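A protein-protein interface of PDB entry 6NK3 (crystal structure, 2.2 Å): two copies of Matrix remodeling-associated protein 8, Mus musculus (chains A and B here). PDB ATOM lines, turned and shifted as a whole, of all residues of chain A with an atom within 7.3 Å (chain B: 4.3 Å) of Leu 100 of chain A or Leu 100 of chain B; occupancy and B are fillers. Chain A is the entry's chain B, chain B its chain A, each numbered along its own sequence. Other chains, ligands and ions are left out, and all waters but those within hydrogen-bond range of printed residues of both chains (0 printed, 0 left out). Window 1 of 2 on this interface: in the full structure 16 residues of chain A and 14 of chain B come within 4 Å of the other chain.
The side-chain carboxylate of Asp 83 of chain B lies within salt-bridge range of the guanidinium group of Arg 102 of chain A.
The guanidinium group of Arg 102 of chain B sits at hydrogen-bond distance from the backbone carbonyl oxygen of Ser 98 of chain A, at 3.2 Å.
Of the 11 printed residues of chain B, 4 touch a printed residue of chain A.
Printed residues of chain B that touch a printed residue of chain A: Asp 83, Leu 86, Leu 100 and Arg 102.
Hydrophobic or aromatic side chains of chain B within 4 Å of the printed part of chain A: Leu 86 and Leu 100.
Of the 21 printed residues of chain A, 7 touch a printed residue of chain B.
Hydrophobic or aromatic side chains of chain A that line the printed part of chain B: Leu 86, Leu 100 and Leu 160.
Among the printed residues, Asp or Glu carboxylates within 4 Å of a Lys or Arg side-chain nitrogen of the other chain: Arg 102 of chain A with Asp 83 of chain B (2.6 Å).
Gln 74 of chain A touches none of the printed residues of chain B.
Leu 99 of chain A touches none of the printed residues of chain B.
Of the printed residues of chain B, Leu 100 of chain A touches Asp 83, Leu 86, Leu 100 and Arg 102.
Of the printed residues of chain B, Arg 102 of chain A touches Asp 83 (2.6 Å).
Of the printed residues of chain A, Asp 83 of chain B touches Leu 86, Leu 100 and Arg 102.
Of the printed residues of chain A, Leu 100 of chain B touches Leu 100.
The nearest printed residue of chain B that does not touch Leu 100 of chain A is Arg 84 of chain B (5.9 Å).
The backbone carbonyl oxygen (O) of Arg 84 of chain A lies within hydrogen-bond range of the backbone NH (N) of Arg 102 of chain A (2.8 Å).
N of Arg 102 of chain B is in hydrogen-bond range of O of Arg 84 of chain B.
NE of Arg 102 of chain A sits at hydrogen-bond distance from O of Asp 83 of chain A (2.7 Å).
The backbone NH (N) of Leu 86 of chain B lies within hydrogen-bond range of the backbone carbonyl oxygen (O) of Leu 100 of chain B, 2.9 Å away.
The side-chain amide oxygen (OE1) of Gln 74 of chain A sits at hydrogen-bond distance from the backbone NH (N) of Leu 87 of chain A (2.8 Å).
The backbone NH (N) of Leu 86 of chain A lies within hydrogen-bond range of the backbone carbonyl oxygen (O) of Leu 100 of chain A, at 2.8 Å.
Among the printed residues, merely in contact across the chains: Ser 88 of chain A with Arg 102 of chain B (3.5 Å), Leu 86 of chain A with Arg 102 of chain B (3.6 Å), Leu 86 of chain A with Asp 83 of chain B (3.6 Å), Leu 160 of chain A with Arg 102 of chain B (3.8 Å), Leu 100 of chain A with Leu 100 of chain B (3.8 Å), Leu 100 of chain A with Leu 86 of chain B (3.9 Å), Leu 87 of chain A with Arg 102 of chain B (3.9 Å), Leu 100 of chain A with Arg 102 of chain B (3.9 Å) and Leu 100 of chain A with Asp 83 of chain B (3.98 Å).
Leu 86 of chain A touches Asp 83 of chain B, but with the chains exchanged Asp 83 of chain A does not touch Leu 86 of chain B (7.4 Å).
Ser 98 of chain A touches Arg 102 of chain B, but with the chains exchanged Arg 102 of chain A does not touch Ser 98 of chain B (9.4 Å).
Leu 100 of chain A touches Asp 83 of chain B, but with the chains exchanged Asp 83 of chain A does not touch Leu 100 of chain B (12.1 Å).
Arg 102 of chain A touches Asp 83 of chain B, but with the chains exchanged Asp 83 of chain A does not touch Arg 102 of chain B (10.5 Å).
Positions printed for both chains: 83, 84, 85, 86, 98, 99, 100, 101, 102, 159 and 160.
Of the 11 pairs that touch across the chains among the printed residues, 1 has its exchanged pair printed and touching as well.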
ATOM      1  N   TRP A  52      21.980 -12.045 -21.077  1.00  0.00           N
ATOM      2  CA  TRP A  52      23.155 -11.385 -21.621  1.00  0.00           C
ATOM      3  C   TRP A  52      24.185 -12.441 -21.989  1.00  0.00           C
ATOM      4  O   TRP A  52      24.523 -13.298 -21.164  1.00  0.00           O
ATOM      5  CB  TRP A  52      23.744 -10.393 -20.617  1.00  0.00           C
ATOM      6  CG  TRP A  52      23.012  -9.085 -20.551  1.00  0.00           C
ATOM      7  CD1 TRP A  52      21.878  -8.813 -19.842  1.00  0.00           C
ATOM      8  CD2 TRP A  52      23.372  -7.866 -21.214  1.00  0.00           C
ATOM      9  NE1 TRP A  52      21.508  -7.502 -20.026  1.00  0.00           N
ATOM     10  CE2 TRP A  52      22.409  -6.899 -20.864  1.00  0.00           C
ATOM     11  CE3 TRP A  52      24.414  -7.499 -22.071  1.00  0.00           C
ATOM     12  CZ2 TRP A  52      22.458  -5.590 -21.337  1.00  0.00           C
ATOM     13  CZ3 TRP A  52      24.460  -6.199 -22.543  1.00  0.00           C
ATOM     14  CH2 TRP A  52      23.488  -5.260 -22.175  1.00  0.00           C
ATOM     15  N   GLN A  74      17.346 -13.207 -10.941  1.00  0.00           N
ATOM     16  CA  GLN A  74      18.421 -13.373 -11.905  1.00  0.00           C
ATOM     17  C   GLN A  74      19.270 -14.590 -11.560  1.00  0.00           C
ATOM     18  O   GLN A  74      19.427 -14.961 -10.393  1.00  0.00           O
ATOM     19  CB  GLN A  74      19.298 -12.121 -11.966  1.00  0.00           C
ATOM     20  CG  GLN A  74      20.357 -12.023 -10.879  1.00  0.00           C
ATOM     21  CD  GLN A  74      21.328 -10.882 -11.114  1.00  0.00           C
ATOM     22  OE1 GLN A  74      20.932  -9.787 -11.511  1.00  0.00           O
ATOM     23  NE2 GLN A  74      22.611 -11.139 -10.880  1.00  0.00           N
ATOM     24  N   ASP A  83      27.043 -11.776  -7.544  1.00  0.00           N
ATOM     25  CA  ASP A  83      27.172 -10.457  -6.927  1.00  0.00           C
ATOM     26  C   ASP A  83      28.077  -9.541  -7.744  1.00  0.00           C
ATOM     27  O   ASP A  83      28.359  -8.412  -7.333  1.00  0.00           O
ATOM     28  CB  ASP A  83      27.701 -10.570  -5.493  1.00  0.00           C
ATOM     29  CG  ASP A  83      26.784 -11.371  -4.594  1.00  0.00           C
ATOM     30  OD1 ASP A  83      25.562 -11.372  -4.840  1.00  0.00           O
ATOM     31  OD2 ASP A  83      27.290 -11.999  -3.639  1.00  0.00           O
ATOM     32  N   ARG A  84      28.527 -10.017  -8.904  1.00  0.00           N
ATOM     33  CA  ARG A  84      29.438  -9.284  -9.773  1.00  0.00           C
ATOM     34  C   ARG A  84      28.752  -8.747 -11.020  1.00  0.00           C
ATOM     35  O   ARG A  84      28.996  -7.601 -11.410  1.00  0.00           O
ATOM     36  CB  ARG A  84      30.611 -10.187 -10.171  1.00  0.00           C
ATOM     37  CG  ARG A  84      31.682  -9.512 -10.999  1.00  0.00           C
ATOM     38  CD  ARG A  84      32.838 -10.462 -11.258  1.00  0.00           C
ATOM     39  NE  ARG A  84      33.821  -9.892 -12.171  1.00  0.00           N
ATOM     40  CZ  ARG A  84      33.785 -10.038 -13.492  1.00  0.00           C
ATOM     41  NH1 ARG A  84      34.725  -9.483 -14.242  1.00  0.00           N
ATOM     42  NH2 ARG A  84      32.814 -10.740 -14.060  1.00  0.00           N
ATOM     43  N   LEU A  85      27.905  -9.549 -11.654  1.00  0.00           N
ATOM     44  CA  LEU A  85      27.021  -9.085 -12.713  1.00  0.00           C
ATOM     45  C   LEU A  85      25.639  -8.868 -12.115  1.00  0.00           C
ATOM     46  O   LEU A  85      25.120  -9.743 -11.412  1.00  0.00           O
ATOM     47  CB  LEU A  85      26.948 -10.092 -13.862  1.00  0.00           C
ATOM     48  CG  LEU A  85      28.264 -10.646 -14.412  1.00  0.00           C
ATOM     49  CD1 LEU A  85      27.989 -11.653 -15.519  1.00  0.00           C
ATOM     50  CD2 LEU A  85      29.161  -9.529 -14.914  1.00  0.00           C
ATOM     51  N   LEU A  86      25.051  -7.704 -12.377  1.00  0.00           N
ATOM     52  CA  LEU A  86      23.779  -7.336 -11.772  1.00  0.00           C
ATOM     53  C   LEU A  86      22.800  -6.862 -12.832  1.00  0.00           C
ATOM     54  O   LEU A  86      23.148  -6.038 -13.685  1.00  0.00           O
ATOM     55  CB  LEU A  86      23.957  -6.242 -10.712  1.00  0.00           C
ATOM     56  CG  LEU A  86      24.459  -6.670  -9.331  1.00  0.00           C
ATOM     57  CD1 LEU A  86      25.971  -6.834  -9.321  1.00  0.00           C
ATOM     58  CD2 LEU A  86      24.010  -5.678  -8.265  1.00  0.00           C
ATOM     59  N   LEU A  87      21.585  -7.391 -12.772  1.00  0.00           N
ATOM     60  CA  LEU A  87      20.440  -6.853 -13.483  1.00  0.00           C
ATOM     61  C   LEU A  87      19.543  -6.110 -12.501  1.00  0.00           C
ATOM     62  O   LEU A  87      19.585  -6.342 -11.290  1.00  0.00           O
ATOM     63  CB  LEU A  87      19.650  -7.966 -14.176  1.00  0.00           C
ATOM     64  CG  LEU A  87      20.424  -8.809 -15.190  1.00  0.00           C
ATOM     65  CD1 LEU A  87      19.555  -9.931 -15.736  1.00  0.00           C
ATOM     66  CD2 LEU A  87      20.939  -7.931 -16.317  1.00  0.00           C
ATOM     67  N   SER A  88      18.739  -5.204 -13.032  1.00  0.00           N
ATOM     68  CA  SER A  88      17.755  -4.528 -12.202  1.00  0.00           C
ATOM     69  C   SER A  88      16.621  -5.495 -11.876  1.00  0.00           C
ATOM     70  O   SER A  88      16.032  -6.080 -12.790  1.00  0.00           O
ATOM     71  CB  SER A  88      17.209  -3.295 -12.911  1.00  0.00           C
ATOM     72  OG  SER A  88      16.062  -2.794 -12.247  1.00  0.00           O
ATOM     73  N   PHE A  97      16.827  -3.293 -19.115  1.00  0.00           N
ATOM     74  CA  PHE A  97      17.509  -4.574 -19.040  1.00  0.00           C
ATOM     75  C   PHE A  97      19.022  -4.415 -19.061  1.00  0.00           C
ATOM     76  O   PHE A  97      19.734  -5.332 -19.482  1.00  0.00           O
ATOM     77  CB  PHE A  97      17.030  -5.479 -20.177  1.00  0.00           C
ATOM     78  CG  PHE A  97      15.537  -5.609 -20.236  1.00  0.00           C
ATOM     79  CD1 PHE A  97      14.880  -6.531 -19.440  1.00  0.00           C
ATOM     80  CD2 PHE A  97      14.787  -4.788 -21.063  1.00  0.00           C
ATOM     81  CE1 PHE A  97      13.504  -6.645 -19.476  1.00  0.00           C
ATOM     82  CE2 PHE A  97      13.408  -4.899 -21.104  1.00  0.00           C
ATOM     83  CZ  PHE A  97      12.768  -5.827 -20.309  1.00  0.00           C
ATOM     84  N   SER A  98      19.519  -3.270 -18.603  1.00  0.00           N
ATOM     85  CA  SER A  98      20.947  -2.997 -18.635  1.00  0.00           C
ATOM     86  C   SER A  98      21.701  -3.943 -17.712  1.00  0.00           C
ATOM     87  O   SER A  98      21.185  -4.393 -16.686  1.00  0.00           O
ATOM     88  CB  SER A  98      21.210  -1.550 -18.224  1.00  0.00           C
ATOM     89  OG  SER A  98      20.477  -0.653 -19.040  1.00  0.00           O
ATOM     90  N   LEU A  99      22.942  -4.236 -18.084  1.00  0.00           N
ATOM     91  CA  LEU A  99      23.809  -5.100 -17.298  1.00  0.00           C
ATOM     92  C   LEU A  99      24.877  -4.263 -16.604  1.00  0.00           C
ATOM     93  O   LEU A  99      25.577  -3.478 -17.251  1.00  0.00           O
ATOM     94  CB  LEU A  99      24.466  -6.168 -18.173  1.00  0.00           C
ATOM     95  CG  LEU A  99      25.486  -7.073 -17.473  1.00  0.00           C
ATOM     96  CD1 LEU A  99      24.823  -7.902 -16.381  1.00  0.00           C
ATOM     97  CD2 LEU A  99      26.193  -7.973 -18.473  1.00  0.00           C
ATOM     98  N   LEU A 100      24.990  -4.427 -15.290  1.00  0.00           N
ATOM     99  CA  LEU A 100      26.017  -3.759 -14.503  1.00  0.00           C
ATOM    100  C   LEU A 100      27.090  -4.773 -14.132  1.00  0.00           C
ATOM    101  O   LEU A 100      26.789  -5.804 -13.519  1.00  0.00           O
ATOM    102  CB  LEU A 100      25.421  -3.125 -13.247  1.00  0.00           C
ATOM    103  CG  LEU A 100      26.438  -2.559 -12.253  1.00  0.00           C
ATOM    104  CD1 LEU A 100      27.135  -1.333 -12.831  1.00  0.00           C
ATOM    105  CD2 LEU A 100      25.769  -2.233 -10.926  1.00  0.00           C
ATOM    106  N   ILE A 101      28.328  -4.489 -14.517  1.00  0.00           N
ATOM    107  CA  ILE A 101      29.484  -5.262 -14.084  1.00  0.00           C
ATOM    108  C   ILE A 101      30.148  -4.479 -12.962  1.00  0.00           C
ATOM    109  O   ILE A 101      30.513  -3.312 -13.146  1.00  0.00           O
ATOM    110  CB  ILE A 101      30.460  -5.522 -15.241  1.00  0.00           C
ATOM    111  CG1 ILE A 101      29.744  -6.221 -16.398  1.00  0.00           C
ATOM    112  CG2 ILE A 101      31.640  -6.354 -14.759  1.00  0.00           C
ATOM    113  CD1 ILE A 101      30.631  -6.485 -17.594  1.00  0.00           C
ATOM    114  N   ARG A 102      30.294  -5.108 -11.796  1.00  0.00           N
ATOM    115  CA  ARG A 102      30.761  -4.378 -10.620  1.00  0.00           C
ATOM    116  C   ARG A 102      32.216  -3.946 -10.768  1.00  0.00           C
ATOM    117  O   ARG A 102      32.587  -2.842 -10.353  1.00  0.00           O
ATOM    118  CB  ARG A 102      30.571  -5.228  -9.363  1.00  0.00           C
ATOM    119  CG  ARG A 102      30.731  -4.452  -8.066  1.00  0.00           C
ATOM    120  CD  ARG A 102      30.568  -5.349  -6.849  1.00  0.00           C
ATOM    121  NE  ARG A 102      29.239  -5.950  -6.773  1.00  0.00           N
ATOM    122  CZ  ARG A 102      28.185  -5.364  -6.215  1.00  0.00           C
ATOM    123  NH1 ARG A 102      28.299  -4.155  -5.682  1.00  0.00           N
ATOM    124  NH2 ARG A 102      27.015  -5.988  -6.187  1.00  0.00           N
ATOM    125  N   ALA A 103      33.055  -4.796 -11.356  1.00  0.00           N
ATOM    126  CA  ALA A 103      34.458  -4.456 -11.580  1.00  0.00           C
ATOM    127  C   ALA A 103      34.932  -5.207 -12.816  1.00  0.00           C
ATOM    128  O   ALA A 103      35.048  -6.436 -12.789  1.00  0.00           O
ATOM    129  CB  ALA A 103      35.315  -4.803 -10.364  1.00  0.00           C
ATOM    130  N   VAL A 104      35.210  -4.472 -13.885  1.00  0.00           N
ATOM    131  CA  VAL A 104      35.562  -5.082 -15.161  1.00  0.00           C
ATOM    132  C   VAL A 104      37.034  -5.469 -15.161  1.00  0.00           C
ATOM    133  O   VAL A 104      37.898  -4.700 -14.722  1.00  0.00           O
ATOM    134  CB  VAL A 104      35.235  -4.125 -16.321  1.00  0.00           C
ATOM    135  CG1 VAL A 104      35.530  -4.785 -17.646  1.00  0.00           C
ATOM    136  CG2 VAL A 104      33.784  -3.709 -16.255  1.00  0.00           C
ATOM    137  N   ALA A 157      37.132  -0.724 -13.101  1.00  0.00           N
ATOM    138  CA  ALA A 157      35.990   0.153 -12.919  1.00  0.00           C
ATOM    139  C   ALA A 157      34.683  -0.600 -13.163  1.00  0.00           C
ATOM    140  O   ALA A 157      34.650  -1.571 -13.925  1.00  0.00           O
ATOM    141  CB  ALA A 157      36.072   1.342 -13.868  1.00  0.00           C
ATOM    142  N   PRO A 158      33.594  -0.181 -12.522  1.00  0.00           N
ATOM    143  CA  PRO A 158      32.284  -0.731 -12.883  1.00  0.00           C
ATOM    144  C   PRO A 158      31.838  -0.214 -14.240  1.00  0.00           C
ATOM    145  O   PRO A 158      32.166   0.903 -14.646  1.00  0.00           O
ATOM    146  CB  PRO A 158      31.367  -0.228 -11.764  1.00  0.00           C
ATOM    147  CG  PRO A 158      32.023   1.034 -11.294  1.00  0.00           C
ATOM    148  CD  PRO A 158      33.503   0.773 -11.403  1.00  0.00           C
ATOM    149  N   ALA A 159      31.081  -1.048 -14.949  1.00  0.00           N
ATOM    150  CA  ALA A 159      30.566  -0.699 -16.265  1.00  0.00           C
ATOM    151  C   ALA A 159      29.089  -1.049 -16.349  1.00  0.00           C
ATOM    152  O   ALA A 159      28.669  -2.119 -15.901  1.00  0.00           O
ATOM    153  CB  ALA A 159      31.330  -1.418 -17.380  1.00  0.00           C
ATOM    154  N   LEU A 160      28.307  -0.138 -16.920  1.00  0.00           N
ATOM    155  CA  LEU A 160      26.890  -0.365 -17.175  1.00  0.00           C
ATOM    156  C   LEU A 160      26.676  -0.372 -18.682  1.00  0.00           C
ATOM    157  O   LEU A 160      26.881   0.649 -19.349  1.00  0.00           O
ATOM    158  CB  LEU A 160      26.016   0.699 -16.512  1.00  0.00           C
ATOM    159  CG  LEU A 160      24.528   0.369 -16.655  1.00  0.00           C
ATOM    160  CD1 LEU A 160      24.051  -0.486 -15.489  1.00  0.00           C
ATOM    161  CD2 LEU A 160      23.675   1.614 -16.804  1.00  0.00           C
ATOM    162  N   MET A 161      26.272  -1.519 -19.217  1.00  0.00           N
ATOM    163  CA  MET A 161      25.913  -1.631 -20.623  1.00  0.00           C
ATOM    164  C   MET A 161      24.404  -1.460 -20.755  1.00  0.00           C
ATOM    165  O   MET A 161      23.633  -2.251 -20.202  1.00  0.00           O
ATOM    166  CB  MET A 161      26.380  -2.971 -21.191  1.00  0.00           C
ATOM    167  CG  MET A 161      27.886  -3.020 -21.432  1.00  0.00           C
ATOM    168  SD  MET A 161      28.521  -4.667 -21.783  1.00  0.00           S
ATOM    169  CE  MET A 161      28.224  -5.482 -20.220  1.00  0.00           C
ATOM    170  N   ASP B  83      24.678  -1.169  -4.313  1.00  0.00           N
ATOM    171  CA  ASP B  83      24.579  -1.639  -5.694  1.00  0.00           C
ATOM    172  C   ASP B  83      24.036  -0.573  -6.639  1.00  0.00           C
ATOM    173  O   ASP B  83      23.711  -0.881  -7.793  1.00  0.00           O
ATOM    174  CB  ASP B  83      23.727  -2.911  -5.800  1.00  0.00           C
ATOM    175  CG  ASP B  83      24.309  -4.070  -5.018  1.00  0.00           C
ATOM    176  OD1 ASP B  83      25.552  -4.183  -4.958  1.00  0.00           O
ATOM    177  OD2 ASP B  83      23.525  -4.866  -4.459  1.00  0.00           O
ATOM    178  N   ARG B  84      23.933   0.671  -6.181  1.00  0.00           N
ATOM    179  CA  ARG B  84      23.440   1.786  -6.978  1.00  0.00           C
ATOM    180  C   ARG B  84      24.481   2.877  -7.173  1.00  0.00           C
ATOM    181  O   ARG B  84      24.611   3.412  -8.276  1.00  0.00           O
ATOM    182  CB  ARG B  84      22.189   2.379  -6.321  1.00  0.00           C
ATOM    183  CG  ARG B  84      21.516   3.487  -7.109  1.00  0.00           C
ATOM    184  CD  ARG B  84      20.233   3.929  -6.426  1.00  0.00           C
ATOM    185  NE  ARG B  84      19.697   5.157  -7.002  1.00  0.00           N
ATOM    186  CZ  ARG B  84      19.997   6.377  -6.569  1.00  0.00           C
ATOM    187  NH1 ARG B  84      20.825   6.538  -5.546  1.00  0.00           N
ATOM    188  NH2 ARG B  84      19.462   7.435  -7.156  1.00  0.00           N
ATOM    189  N   LEU B  85      25.223   3.217  -6.123  1.00  0.00           N
ATOM    190  CA  LEU B  85      26.376   4.102  -6.212  1.00  0.00           C
ATOM    191  C   LEU B  85      27.629   3.243  -6.106  1.00  0.00           C
ATOM    192  O   LEU B  85      27.826   2.554  -5.100  1.00  0.00           O
ATOM    193  CB  LEU B  85      26.349   5.154  -5.103  1.00  0.00           C
ATOM    194  CG  LEU B  85      25.558   6.455  -5.277  1.00  0.00           C
ATOM    195  CD1 LEU B  85      24.168   6.219  -5.835  1.00  0.00           C
ATOM    196  CD2 LEU B  85      25.467   7.172  -3.943  1.00  0.00           C
ATOM    197  N   LEU B  86      28.469   3.272  -7.138  1.00  0.00           N
ATOM    198  CA  LEU B  86      29.597   2.356  -7.219  1.00  0.00           C
ATOM    199  C   LEU B  86      30.884   3.100  -7.543  1.00  0.00           C
ATOM    200  O   LEU B  86      30.912   3.976  -8.413  1.00  0.00           O
ATOM    201  CB  LEU B  86      29.357   1.268  -8.273  1.00  0.00           C
ATOM    202  CG  LEU B  86      28.159   0.348  -8.031  1.00  0.00           C
ATOM    203  CD1 LEU B  86      26.934   0.849  -8.785  1.00  0.00           C
ATOM    204  CD2 LEU B  86      28.497  -1.085  -8.417  1.00  0.00           C
ATOM    205  N   SER B  98      36.176   7.893 -10.058  1.00  0.00           N
ATOM    206  CA  SER B  98      34.879   8.279 -10.592  1.00  0.00           C
ATOM    207  C   SER B  98      33.758   7.546  -9.866  1.00  0.00           C
ATOM    208  O   SER B  98      33.938   6.436  -9.357  1.00  0.00           O
ATOM    209  CB  SER B  98      34.808   7.979 -12.087  1.00  0.00           C
ATOM    210  OG  SER B  98      35.933   8.506 -12.766  1.00  0.00           O
ATOM    211  N   LEU B  99      32.591   8.180  -9.820  1.00  0.00           N
ATOM    212  CA  LEU B  99      31.417   7.624  -9.162  1.00  0.00           C
ATOM    213  C   LEU B  99      30.356   7.302 -10.206  1.00  0.00           C
ATOM    214  O   LEU B  99      29.942   8.180 -10.971  1.00  0.00           O
ATOM    215  CB  LEU B  99      30.861   8.594  -8.122  1.00  0.00           C
ATOM    216  CG  LEU B  99      29.525   8.185  -7.499  1.00  0.00           C
ATOM    217  CD1 LEU B  99      29.684   6.938  -6.640  1.00  0.00           C
ATOM    218  CD2 LEU B  99      28.929   9.330  -6.690  1.00  0.00           C
ATOM    219  N   LEU B 100      29.910   6.051 -10.223  1.00  0.00           N
ATOM    220  CA  LEU B 100      28.857   5.607 -11.124  1.00  0.00           C
ATOM    221  C   LEU B 100      27.549   5.513 -10.350  1.00  0.00           C
ATOM    222  O   LEU B 100      27.453   4.761  -9.374  1.00  0.00           O
ATOM    223  CB  LEU B 100      29.205   4.257 -11.753  1.00  0.00           C
ATOM    224  CG  LEU B 100      28.107   3.655 -12.629  1.00  0.00           C
ATOM    225  CD1 LEU B 100      27.836   4.551 -13.830  1.00  0.00           C
ATOM    226  CD2 LEU B 100      28.468   2.243 -13.072  1.00  0.00           C
ATOM    227  N   ILE B 101      26.556   6.288 -10.774  1.00  0.00           N
ATOM    228  CA  ILE B 101      25.188   6.154 -10.293  1.00  0.00           C
ATOM    229  C   ILE B 101      24.445   5.299 -11.308  1.00  0.00           C
ATOM    230  O   ILE B 101      24.312   5.689 -12.474  1.00  0.00           O
ATOM    231  CB  ILE B 101      24.513   7.523 -10.110  1.00  0.00           C
ATOM    232  CG1 ILE B 101      25.379   8.431  -9.232  1.00  0.00           C
ATOM    233  CG2 ILE B 101      23.126   7.357  -9.507  1.00  0.00           C
ATOM    234  CD1 ILE B 101      24.704   9.730  -8.855  1.00  0.00           C
ATOM    235  N   ARG B 102      23.974   4.129 -10.872  1.00  0.00           N
ATOM    236  CA  ARG B 102      23.424   3.151 -11.809  1.00  0.00           C
ATOM    237  C   ARG B 102      22.233   3.723 -12.571  1.00  0.00           C
ATOM    238  O   ARG B 102      22.134   3.578 -13.794  1.00  0.00           O
ATOM    239  CB  ARG B 102      23.023   1.880 -11.063  1.00  0.00           C
ATOM    240  CG  ARG B 102      22.880   0.670 -11.960  1.00  0.00           C
ATOM    241  CD  ARG B 102      21.961  -0.366 -11.349  1.00  0.00           C
ATOM    242  NE  ARG B 102      21.956  -1.599 -12.126  1.00  0.00           N
ATOM    243  CZ  ARG B 102      21.249  -1.782 -13.237  1.00  0.00           C
ATOM    244  NH1 ARG B 102      20.482  -0.809 -13.709  1.00  0.00           N
ATOM    245  NH2 ARG B 102      21.312  -2.942 -13.876  1.00  0.00           N
ATOM    246  N   ALA B 159      24.717   7.920 -14.547  1.00  0.00           N
ATOM    247  CA  ALA B 159      25.559   9.107 -14.487  1.00  0.00           C
ATOM    248  C   ALA B 159      26.944   8.694 -14.020  1.00  0.00           C
ATOM    249  O   ALA B 159      27.101   8.197 -12.899  1.00  0.00           O
ATOM    250  CB  ALA B 159      24.972  10.165 -13.552  1.00  0.00           C
ATOM    251  N   LEU B 160      27.938   8.885 -14.880  1.00  0.00           N
ATOM    252  CA  LEU B 160      29.334   8.654 -14.527  1.00  0.00           C
ATOM    253  C   LEU B 160      29.964  10.013 -14.242  1.00  0.00           C
ATOM    254  O   LEU B 160      30.248  10.787 -15.160  1.00  0.00           O
ATOM    255  CB  LEU B 160      30.073   7.914 -15.635  1.00  0.00           C
ATOM    256  CG  LEU B 160      31.552   7.695 -15.318  1.00  0.00           C
ATOM    257  CD1 LEU B 160      31.707   6.767 -14.123  1.00  0.00           C
ATOM    258  CD2 LEU B 160      32.302   7.160 -16.525  1.00  0.00           C
